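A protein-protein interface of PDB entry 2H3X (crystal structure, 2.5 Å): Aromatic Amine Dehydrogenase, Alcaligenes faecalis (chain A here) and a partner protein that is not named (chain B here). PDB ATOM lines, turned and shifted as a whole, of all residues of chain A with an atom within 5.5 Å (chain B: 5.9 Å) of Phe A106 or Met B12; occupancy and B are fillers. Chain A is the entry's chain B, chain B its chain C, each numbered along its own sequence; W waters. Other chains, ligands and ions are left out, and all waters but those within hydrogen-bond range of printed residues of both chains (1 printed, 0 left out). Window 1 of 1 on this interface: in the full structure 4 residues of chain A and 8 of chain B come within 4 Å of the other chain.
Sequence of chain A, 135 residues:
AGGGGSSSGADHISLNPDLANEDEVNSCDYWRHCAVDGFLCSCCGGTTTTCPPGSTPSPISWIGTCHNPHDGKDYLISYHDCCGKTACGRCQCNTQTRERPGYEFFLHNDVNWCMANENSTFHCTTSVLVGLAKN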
ATOM      1  N   PRO A  59      -7.201   4.887  -8.520  1.00  0.00           N
ATOM      2  CA  PRO A  59      -6.364   5.980  -9.016  1.00  0.00           C
ATOM      3  C   PRO A  59      -4.996   5.449  -9.431  1.00  0.00           C
ATOM      4  O   PRO A  59      -4.357   5.988 -10.322  1.00  0.00           O
ATOM      5  CB  PRO A  59      -6.283   6.921  -7.819  1.00  0.00           C
ATOM      6  CG  PRO A  59      -6.320   5.974  -6.653  1.00  0.00           C
ATOM      7  CD  PRO A  59      -7.404   4.995  -7.063  1.00  0.00           C
ATOM      8  N   ILE A  60      -4.556   4.377  -8.785  1.00  0.00           N
ATOM      9  CA  ILE A  60      -3.263   3.794  -9.105  1.00  0.00           C
ATOM     10  C   ILE A  60      -3.409   2.543  -9.951  1.00  0.00           C
ATOM     11  O   ILE A  60      -4.520   2.098 -10.225  1.00  0.00           O
ATOM     12  CB  ILE A  60      -2.481   3.463  -7.829  1.00  0.00           C
ATOM     13  CG1 ILE A  60      -3.317   2.553  -6.925  1.00  0.00           C
ATOM     14  CG2 ILE A  60      -2.112   4.754  -7.118  1.00  0.00           C
ATOM     15  CD1 ILE A  60      -2.651   2.203  -5.613  1.00  0.00           C
ATOM     16  N   SER A  61      -2.281   1.976 -10.360  1.00  0.00           N
ATOM     17  CA  SER A  61      -2.297   0.789 -11.203  1.00  0.00           C
ATOM     18  C   SER A  61      -0.885   0.268 -11.378  1.00  0.00           C
ATOM     19  O   SER A  61       0.067   0.892 -10.923  1.00  0.00           O
ATOM     20  CB  SER A  61      -2.830   1.149 -12.583  1.00  0.00           C
ATOM     21  OG  SER A  61      -1.902   1.997 -13.239  1.00  0.00           O
ATOM     22  N   TRQ A  62      -0.762  -0.884 -12.031  1.00  0.00           N
ATOM     23  CA  TRQ A  62       0.546  -1.445 -12.323  1.00  0.00           C
ATOM     24  C   TRQ A  62       0.740  -1.230 -13.832  1.00  0.00           C
ATOM     25  O   TRQ A  62      -0.231  -1.220 -14.599  1.00  0.00           O
ATOM     26  CB  TRQ A  62       0.626  -2.923 -11.892  1.00  0.00           C
ATOM     27  CG  TRQ A  62      -0.398  -3.885 -12.458  1.00  0.00           C
ATOM     28  CD1 TRQ A  62      -0.297  -4.538 -13.650  1.00  0.00           C
ATOM     29  NE1 TRQ A  62      -1.350  -5.386 -13.823  1.00  0.00           N
ATOM     30  CE2 TRQ A  62      -2.178  -5.301 -12.737  1.00  0.00           C
ATOM     31  CZ2 TRQ A  62      -3.376  -5.985 -12.486  1.00  0.00           C
ATOM     32  CH2 TRQ A  62      -4.038  -5.713 -11.314  1.00  0.00           C
ATOM     33  CZ3 TRQ A  62      -3.530  -4.790 -10.384  1.00  0.00           C
ATOM     34  CE3 TRQ A  62      -2.332  -4.108 -10.623  1.00  0.00           C
ATOM     35  CD2 TRQ A  62      -1.624  -4.358 -11.831  1.00  0.00           C
ATOM     36  O6  TRQ A  62      -5.127  -6.247 -11.021  1.00  0.00           O
ATOM     37  O7  TRQ A  62      -3.735  -6.795 -13.346  1.00  0.00           O
ATOM     38  N   ILE A  63       1.981  -1.009 -14.251  1.00  0.00           N
ATOM     39  CA  ILE A  63       2.269  -0.731 -15.655  1.00  0.00           C
ATOM     40  C   ILE A  63       2.898  -1.868 -16.432  1.00  0.00           C
ATOM     41  O   ILE A  63       3.811  -2.542 -15.949  1.00  0.00           O
ATOM     42  CB  ILE A  63       3.207   0.495 -15.809  1.00  0.00           C
ATOM     43  CG1 ILE A  63       2.601   1.725 -15.127  1.00  0.00           C
ATOM     44  CG2 ILE A  63       3.434   0.785 -17.280  1.00  0.00           C
ATOM     45  CD1 ILE A  63       1.253   2.149 -15.688  1.00  0.00           C
ATOM     46  N   GLU A 104      10.059  -2.981  -7.664  1.00  0.00           N
ATOM     47  CA  GLU A 104       9.737  -2.157  -8.832  1.00  0.00           C
ATOM     48  C   GLU A 104       8.221  -2.161  -8.758  1.00  0.00           C
ATOM     49  O   GLU A 104       7.531  -2.601  -9.677  1.00  0.00           O
ATOM     50  CB  GLU A 104      10.194  -2.815 -10.136  1.00  0.00           C
ATOM     51  CG  GLU A 104      11.693  -2.810 -10.354  1.00  0.00           C
ATOM     52  CD  GLU A 104      12.065  -2.437 -11.782  1.00  0.00           C
ATOM     53  OE1 GLU A 104      11.890  -1.252 -12.150  1.00  0.00           O
ATOM     54  OE2 GLU A 104      12.524  -3.327 -12.535  1.00  0.00           O
ATOM     55  N   PHE A 105       7.719  -1.664  -7.634  1.00  0.00           N
ATOM     56  CA  PHE A 105       6.301  -1.656  -7.323  1.00  0.00           C
ATOM     57  C   PHE A 105       5.269  -1.399  -8.420  1.00  0.00           C
ATOM     58  O   PHE A 105       4.333  -2.193  -8.586  1.00  0.00           O
ATOM     59  CB  PHE A 105       6.039  -0.707  -6.146  1.00  0.00           C
ATOM     60  CG  PHE A 105       4.896  -1.142  -5.269  1.00  0.00           C
ATOM     61  CD1 PHE A 105       4.897  -2.407  -4.683  1.00  0.00           C
ATOM     62  CD2 PHE A 105       3.819  -0.297  -5.033  1.00  0.00           C
ATOM     63  CE1 PHE A 105       3.841  -2.828  -3.875  1.00  0.00           C
ATOM     64  CE2 PHE A 105       2.748  -0.704  -4.222  1.00  0.00           C
ATOM     65  CZ  PHE A 105       2.761  -1.972  -3.642  1.00  0.00           C
ATOM     66  N   PHE A 106       5.416  -0.318  -9.176  1.00  0.00           N
ATOM     67  CA  PHE A 106       4.419  -0.021 -10.196  1.00  0.00           C
ATOM     68  C   PHE A 106       4.468  -0.819 -11.493  1.00  0.00           C
ATOM     69  O   PHE A 106       3.778  -0.505 -12.455  1.00  0.00           O
ATOM     70  CB  PHE A 106       4.399   1.482 -10.465  1.00  0.00           C
ATOM     71  CG  PHE A 106       4.052   2.284  -9.248  1.00  0.00           C
ATOM     72  CD1 PHE A 106       5.039   2.953  -8.530  1.00  0.00           C
ATOM     73  CD2 PHE A 106       2.744   2.304  -8.768  1.00  0.00           C
ATOM     74  CE1 PHE A 106       4.726   3.626  -7.344  1.00  0.00           C
ATOM     75  CE2 PHE A 106       2.421   2.971  -7.587  1.00  0.00           C
ATOM     76  CZ  PHE A 106       3.415   3.634  -6.871  1.00  0.00           C
ATOM     77  N   LEU A 107       5.275  -1.871 -11.504  1.00  0.00           N
ATOM     78  CA  LEU A 107       5.368  -2.744 -12.665  1.00  0.00           C
ATOM     79  C   LEU A 107       5.006  -4.134 -12.153  1.00  0.00           C
ATOM     80  O   LEU A 107       5.062  -5.111 -12.894  1.00  0.00           O
ATOM     81  CB  LEU A 107       6.798  -2.769 -13.227  1.00  0.00           C
ATOM     82  CG  LEU A 107       7.541  -1.461 -13.544  1.00  0.00           C
ATOM     83  CD1 LEU A 107       8.782  -1.787 -14.374  1.00  0.00           C
ATOM     84  CD2 LEU A 107       6.650  -0.496 -14.313  1.00  0.00           C
ATOM     85  N   HIS A 108       4.622  -4.201 -10.881  1.00  0.00           N
ATOM     86  CA  HIS A 108       4.285  -5.460 -10.208  1.00  0.00           C
ATOM     87  C   HIS A 108       2.775  -5.748 -10.154  1.00  0.00           C
ATOM     88  O   HIS A 108       1.991  -4.889  -9.725  1.00  0.00           O
ATOM     89  CB  HIS A 108       4.862  -5.419  -8.785  1.00  0.00           C
ATOM     90  CG  HIS A 108       4.785  -6.719  -8.052  1.00  0.00           C
ATOM     91  ND1 HIS A 108       4.352  -6.809  -6.747  1.00  0.00           N
ATOM     92  CD2 HIS A 108       5.117  -7.977  -8.425  1.00  0.00           C
ATOM     93  CE1 HIS A 108       4.418  -8.065  -6.348  1.00  0.00           C
ATOM     94  NE2 HIS A 108       4.879  -8.795  -7.347  1.00  0.00           N
ATOM     95  N   TRP A 113      -4.312  -3.575  -6.833  1.00  0.00           N
ATOM     96  CA  TRP A 113      -4.238  -2.155  -7.152  1.00  0.00           C
ATOM     97  C   TRP A 113      -5.477  -1.363  -6.716  1.00  0.00           C
ATOM     98  O   TRP A 113      -5.637  -0.194  -7.069  1.00  0.00           O
ATOM     99  CB  TRP A 113      -3.917  -1.962  -8.650  1.00  0.00           C
ATOM    100  CG  TRP A 113      -2.431  -2.185  -8.916  1.00  0.00           C
ATOM    101  CD1 TRP A 113      -1.835  -3.195  -9.664  1.00  0.00           C
ATOM    102  CD2 TRP A 113      -1.358  -1.458  -8.312  1.00  0.00           C
ATOM    103  NE1 TRP A 113      -0.473  -3.131  -9.530  1.00  0.00           N
ATOM    104  CE2 TRP A 113      -0.149  -2.078  -8.714  1.00  0.00           C
ATOM    105  CE3 TRP A 113      -1.297  -0.342  -7.466  1.00  0.00           C
ATOM    106  CZ2 TRP A 113       1.107  -1.619  -8.297  1.00  0.00           C
ATOM    107  CZ3 TRP A 113      -0.046   0.117  -7.049  1.00  0.00           C
ATOM    108  CH2 TRP A 113       1.139  -0.524  -7.467  1.00  0.00           C
ATOM    109  N   ASN B   9      -1.506  14.113 -10.303  1.00  0.00           N
ATOM    110  CA  ASN B   9      -2.725  13.529  -9.743  1.00  0.00           C
ATOM    111  C   ASN B   9      -2.487  12.232  -8.974  1.00  0.00           C
ATOM    112  O   ASN B   9      -1.361  11.727  -8.910  1.00  0.00           O
ATOM    113  CB  ASN B   9      -3.744  13.272 -10.857  1.00  0.00           C
ATOM    114  CG  ASN B   9      -3.146  12.524 -12.034  1.00  0.00           C
ATOM    115  OD1 ASN B   9      -2.357  11.599 -11.858  1.00  0.00           O
ATOM    116  ND2 ASN B   9      -3.531  12.918 -13.243  1.00  0.00           N
ATOM    117  N   ASP B  10      -3.558  11.699  -8.390  1.00  0.00           N
ATOM    118  CA  ASP B  10      -3.474  10.456  -7.633  1.00  0.00           C
ATOM    119  C   ASP B  10      -3.193   9.286  -8.565  1.00  0.00           C
ATOM    120  O   ASP B  10      -2.900   8.180  -8.115  1.00  0.00           O
ATOM    121  CB  ASP B  10      -4.776  10.192  -6.880  1.00  0.00           C
ATOM    122  CG  ASP B  10      -5.003  11.163  -5.741  1.00  0.00           C
ATOM    123  OD1 ASP B  10      -4.064  11.389  -4.953  1.00  0.00           O
ATOM    124  OD2 ASP B  10      -6.126  11.690  -5.623  1.00  0.00           O
ATOM    125  N   SER B  11      -3.278   9.542  -9.867  1.00  0.00           N
ATOM    126  CA  SER B  11      -3.046   8.509 -10.864  1.00  0.00           C
ATOM    127  C   SER B  11      -1.589   8.445 -11.291  1.00  0.00           C
ATOM    128  O   SER B  11      -1.245   7.748 -12.247  1.00  0.00           O
ATOM    129  CB  SER B  11      -3.936   8.747 -12.085  1.00  0.00           C
ATOM    130  OG  SER B  11      -5.303   8.807 -11.711  1.00  0.00           O
ATOM    131  N   MET B  12      -0.739   9.183 -10.584  1.00  0.00           N
ATOM    132  CA  MET B  12       0.694   9.191 -10.868  1.00  0.00           C
ATOM    133  C   MET B  12       1.019   9.741 -12.256  1.00  0.00           C
ATOM    134  O   MET B  12       1.775   9.132 -13.014  1.00  0.00           O
ATOM    135  CB  MET B  12       1.232   7.769 -10.737  1.00  0.00           C
ATOM    136  CG  MET B  12       2.739   7.642 -10.612  1.00  0.00           C
ATOM    137  SD  MET B  12       3.157   5.978 -10.029  1.00  0.00           S
ATOM    138  CE  MET B  12       1.916   5.830  -8.697  1.00  0.00           C
ATOM    139  N   GLN B  13       0.458  10.898 -12.585  1.00  0.00           N
ATOM    140  CA  GLN B  13       0.703  11.496 -13.889  1.00  0.00           C
ATOM    141  C   GLN B  13       0.955  12.988 -13.812  1.00  0.00           C
ATOM    142  O   GLN B  13       0.472  13.672 -12.910  1.00  0.00           O
ATOM    143  CB  GLN B  13      -0.493  11.276 -14.816  1.00  0.00           C
ATOM    144  CG  GLN B  13      -0.909   9.836 -15.017  1.00  0.00           C
ATOM    145  CD  GLN B  13      -2.207   9.725 -15.797  1.00  0.00           C
ATOM    146  OE1 GLN B  13      -3.260  10.202 -15.356  1.00  0.00           O
ATOM    147  NE2 GLN B  13      -2.138   9.100 -16.967  1.00  0.00           N
ATOM    148  N   PHE B  14       1.716  13.479 -14.783  1.00  0.00           N
ATOM    149  CA  PHE B  14       2.021  14.897 -14.907  1.00  0.00           C
ATOM    150  C   PHE B  14       1.147  15.378 -16.059  1.00  0.00           C
ATOM    151  O   PHE B  14       0.940  14.641 -17.026  1.00  0.00           O
ATOM    152  CB  PHE B  14       3.495  15.093 -15.262  1.00  0.00           C
ATOM    153  CG  PHE B  14       4.404  15.217 -14.069  1.00  0.00           C
ATOM    154  CD1 PHE B  14       5.738  14.821 -14.154  1.00  0.00           C
ATOM    155  CD2 PHE B  14       3.944  15.768 -12.876  1.00  0.00           C
ATOM    156  CE1 PHE B  14       6.603  14.975 -13.073  1.00  0.00           C
ATOM    157  CE2 PHE B  14       4.802  15.928 -11.789  1.00  0.00           C
ATOM    158  CZ  PHE B  14       6.135  15.530 -11.890  1.00  0.00           C
ATOM    159  N   MET B  43       1.197   9.255  -2.008  1.00  0.00           N
ATOM    160  CA  MET B  43       1.263   9.577  -3.425  1.00  0.00           C
ATOM    161  C   MET B  43       1.848  10.962  -3.648  1.00  0.00           C
ATOM    162  O   MET B  43       1.474  11.659  -4.590  1.00  0.00           O
ATOM    163  CB  MET B  43      -0.146   9.500  -4.024  1.00  0.00           C
ATOM    164  CG  MET B  43      -0.250   9.778  -5.510  1.00  0.00           C
ATOM    165  SD  MET B  43       0.694   8.614  -6.493  1.00  0.00           S
ATOM    166  CE  MET B  43      -0.298   7.182  -6.338  1.00  0.00           C
ATOM    167  N   HIS B  45       4.214  14.027  -4.773  1.00  0.00           N
ATOM    168  CA  HIS B  45       4.935  14.278  -6.021  1.00  0.00           C
ATOM    169  C   HIS B  45       5.907  15.436  -5.842  1.00  0.00           C
ATOM    170  O   HIS B  45       5.751  16.271  -4.953  1.00  0.00           O
ATOM    171  CB  HIS B  45       3.984  14.665  -7.160  1.00  0.00           C
ATOM    172  CG  HIS B  45       2.933  13.643  -7.470  1.00  0.00           C
ATOM    173  ND1 HIS B  45       3.231  12.366  -7.882  1.00  0.00           N
ATOM    174  CD2 HIS B  45       1.582  13.735  -7.476  1.00  0.00           C
ATOM    175  CE1 HIS B  45       2.111  11.711  -8.132  1.00  0.00           C
ATOM    176  NE2 HIS B  45       1.094  12.522  -7.893  1.00  0.00           N
ATOM    177  N   PRO B 114       9.634   7.559  -4.698  1.00  0.00           N
ATOM    178  CA  PRO B 114       9.773   6.121  -4.935  1.00  0.00           C
ATOM    179  C   PRO B 114       8.854   5.465  -5.970  1.00  0.00           C
ATOM    180  O   PRO B 114       7.648   5.302  -5.754  1.00  0.00           O
ATOM    181  CB  PRO B 114       9.613   5.541  -3.539  1.00  0.00           C
ATOM    182  CG  PRO B 114      10.347   6.546  -2.721  1.00  0.00           C
ATOM    183  CD  PRO B 114       9.798   7.852  -3.263  1.00  0.00           C
ATOM    184  N   GLY B 115       9.454   5.100  -7.100  1.00  0.00           N
ATOM    185  CA  GLY B 115       8.732   4.436  -8.168  1.00  0.00           C
ATOM    186  C   GLY B 115       7.991   5.265  -9.204  1.00  0.00           C
ATOM    187  O   GLY B 115       7.548   4.711 -10.209  1.00  0.00           O
ATOM    188  N   HIS B 116       7.862   6.573  -8.994  1.00  0.00           N
ATOM    189  CA  HIS B 116       7.124   7.418  -9.932  1.00  0.00           C
ATOM    190  C   HIS B 116       7.849   7.870 -11.203  1.00  0.00           C
ATOM    191  O   HIS B 116       7.207   8.097 -12.228  1.00  0.00           O
ATOM    192  CB  HIS B 116       6.588   8.659  -9.211  1.00  0.00           C
ATOM    193  CG  HIS B 116       5.609   8.358  -8.120  1.00  0.00           C
ATOM    194  ND1 HIS B 116       4.906   9.340  -7.459  1.00  0.00           N
ATOM    195  CD2 HIS B 116       5.219   7.183  -7.570  1.00  0.00           C
ATOM    196  CE1 HIS B 116       4.125   8.787  -6.550  1.00  0.00           C
ATOM    197  NE2 HIS B 116       4.295   7.480  -6.596  1.00  0.00           N
ATOM    198  N   SER B 118       9.258   6.442 -13.499  1.00  0.00           N
ATOM    199  CA  SER B 118       9.042   5.610 -14.680  1.00  0.00           C
ATOM    200  C   SER B 118       7.990   6.218 -15.604  1.00  0.00           C
ATOM    201  O   SER B 118       8.110   6.140 -16.827  1.00  0.00           O
ATOM    202  CB  SER B 118       8.593   4.209 -14.269  1.00  0.00           C
ATOM    203  OG  SER B 118       7.277   4.241 -13.743  1.00  0.00           O
ATOM    204  N   ILE B 119       6.959   6.815 -15.016  1.00  0.00           N
ATOM    205  CA  ILE B 119       5.887   7.429 -15.794  1.00  0.00           C
ATOM    206  C   ILE B 119       5.873   8.946 -15.689  1.00  0.00           C
ATOM    207  O   ILE B 119       5.607   9.637 -16.671  1.00  0.00           O
ATOM    208  CB  ILE B 119       4.496   6.886 -15.364  1.00  0.00           C
ATOM    209  CG1 ILE B 119       4.235   5.549 -16.057  1.00  0.00           C
ATOM    210  CG2 ILE B 119       3.392   7.898 -15.690  1.00  0.00           C
ATOM    211  CD1 ILE B 119       2.840   5.014 -15.846  1.00  0.00           C
ATOM    212  N   MET B 120       6.150   9.464 -14.498  1.00  0.00           N
ATOM    213  CA  MET B 120       6.160  10.903 -14.290  1.00  0.00           C
ATOM    214  C   MET B 120       7.505  11.492 -14.684  1.00  0.00           C
ATOM    215  O   MET B 120       8.202  12.104 -13.876  1.00  0.00           O
ATOM    216  CB  MET B 120       5.830  11.214 -12.834  1.00  0.00           C
ATOM    217  CG  MET B 120       4.455  10.716 -12.436  1.00  0.00           C
ATOM    218  SD  MET B 120       4.032  11.161 -10.769  1.00  0.00           S
ATOM    219  CE  MET B 120       3.651  12.895 -10.993  1.00  0.00           C
HETATM  220  O   HOH W   1       0.146   4.177 -10.740  1.00  0.00           O
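The side-chain hydroxyl of Ser B11 sits close to the backbone carbonyl oxygen of Pro A59 (3.3 Å).
The backbone carbonyl oxygen (O) of Asp B10 lies close to the backbone carbonyl oxygen (O) of Pro A59 (3.4 Å).
The backbone carbonyl oxygen (O) of Phe A106 sits at hydrogen-bond distance from the backbone NH (N) of Ile A63 (2.6 Å).
The side-chain amide oxygen of Asn B9 lies close to the backbone NH of Ser B11, 3.0 Å away.
The backbone NH of Met B12 is in hydrogen-bond range of the side-chain amide oxygen of Asn B9.
The backbone carbonyl oxygen (O) of Met B43 lies within hydrogen-bond range of a ring nitrogen (NE2) of His B45 (3.4 Å).
SD of Met B43 sits close to NE2 of His B116 (3.8 Å).
Among the printed residues, merely in contact across the chains: Phe A106 with Met B12 (3.1 Å), Ile A60 with Met B43 (3.1 Å), Ile A63 with Ile B119 (3.3 Å), Phe A106 with Gly B115 (3.5 Å), Phe A106 with His B116 (3.6 Å), Ile A60 with Asp B10 (3.7 Å) and Phe A106 with Pro B114 (3.7 Å).
Printed residues of chain B within 4 Å of Ile A60: Asp B10 (3.7 Å) and Met B43 (3.1 Å).
Of chain B, only Met B12, Pro B114, Gly B115 and His B116 come within 4 Å of Phe A106.
Of chain A, only Phe A106 (3.1 Å) comes within 4 Å of Met B12.
Printed residues of chain A within 4 Å of Pro B114: Phe A106.
Of the 14 printed residues of chain B, 8 touch a printed residue of chain A.
Of the 11 printed residues of chain A, 4 touch a printed residue of chain B.
Along chain A the printed residues that touch a printed residue of chain B span positions 59 to 106.
Among the printed residues, 9 pairs touch across the chains.
Among the printed residues, no Asp or Glu carboxylate lies within 4 Å of a Lys or Arg side-chain nitrogen of the other chain.
Water W1 bridges the backbone carbonyl oxygen of Ser A61 and the side-chain sulfur of Met B12.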
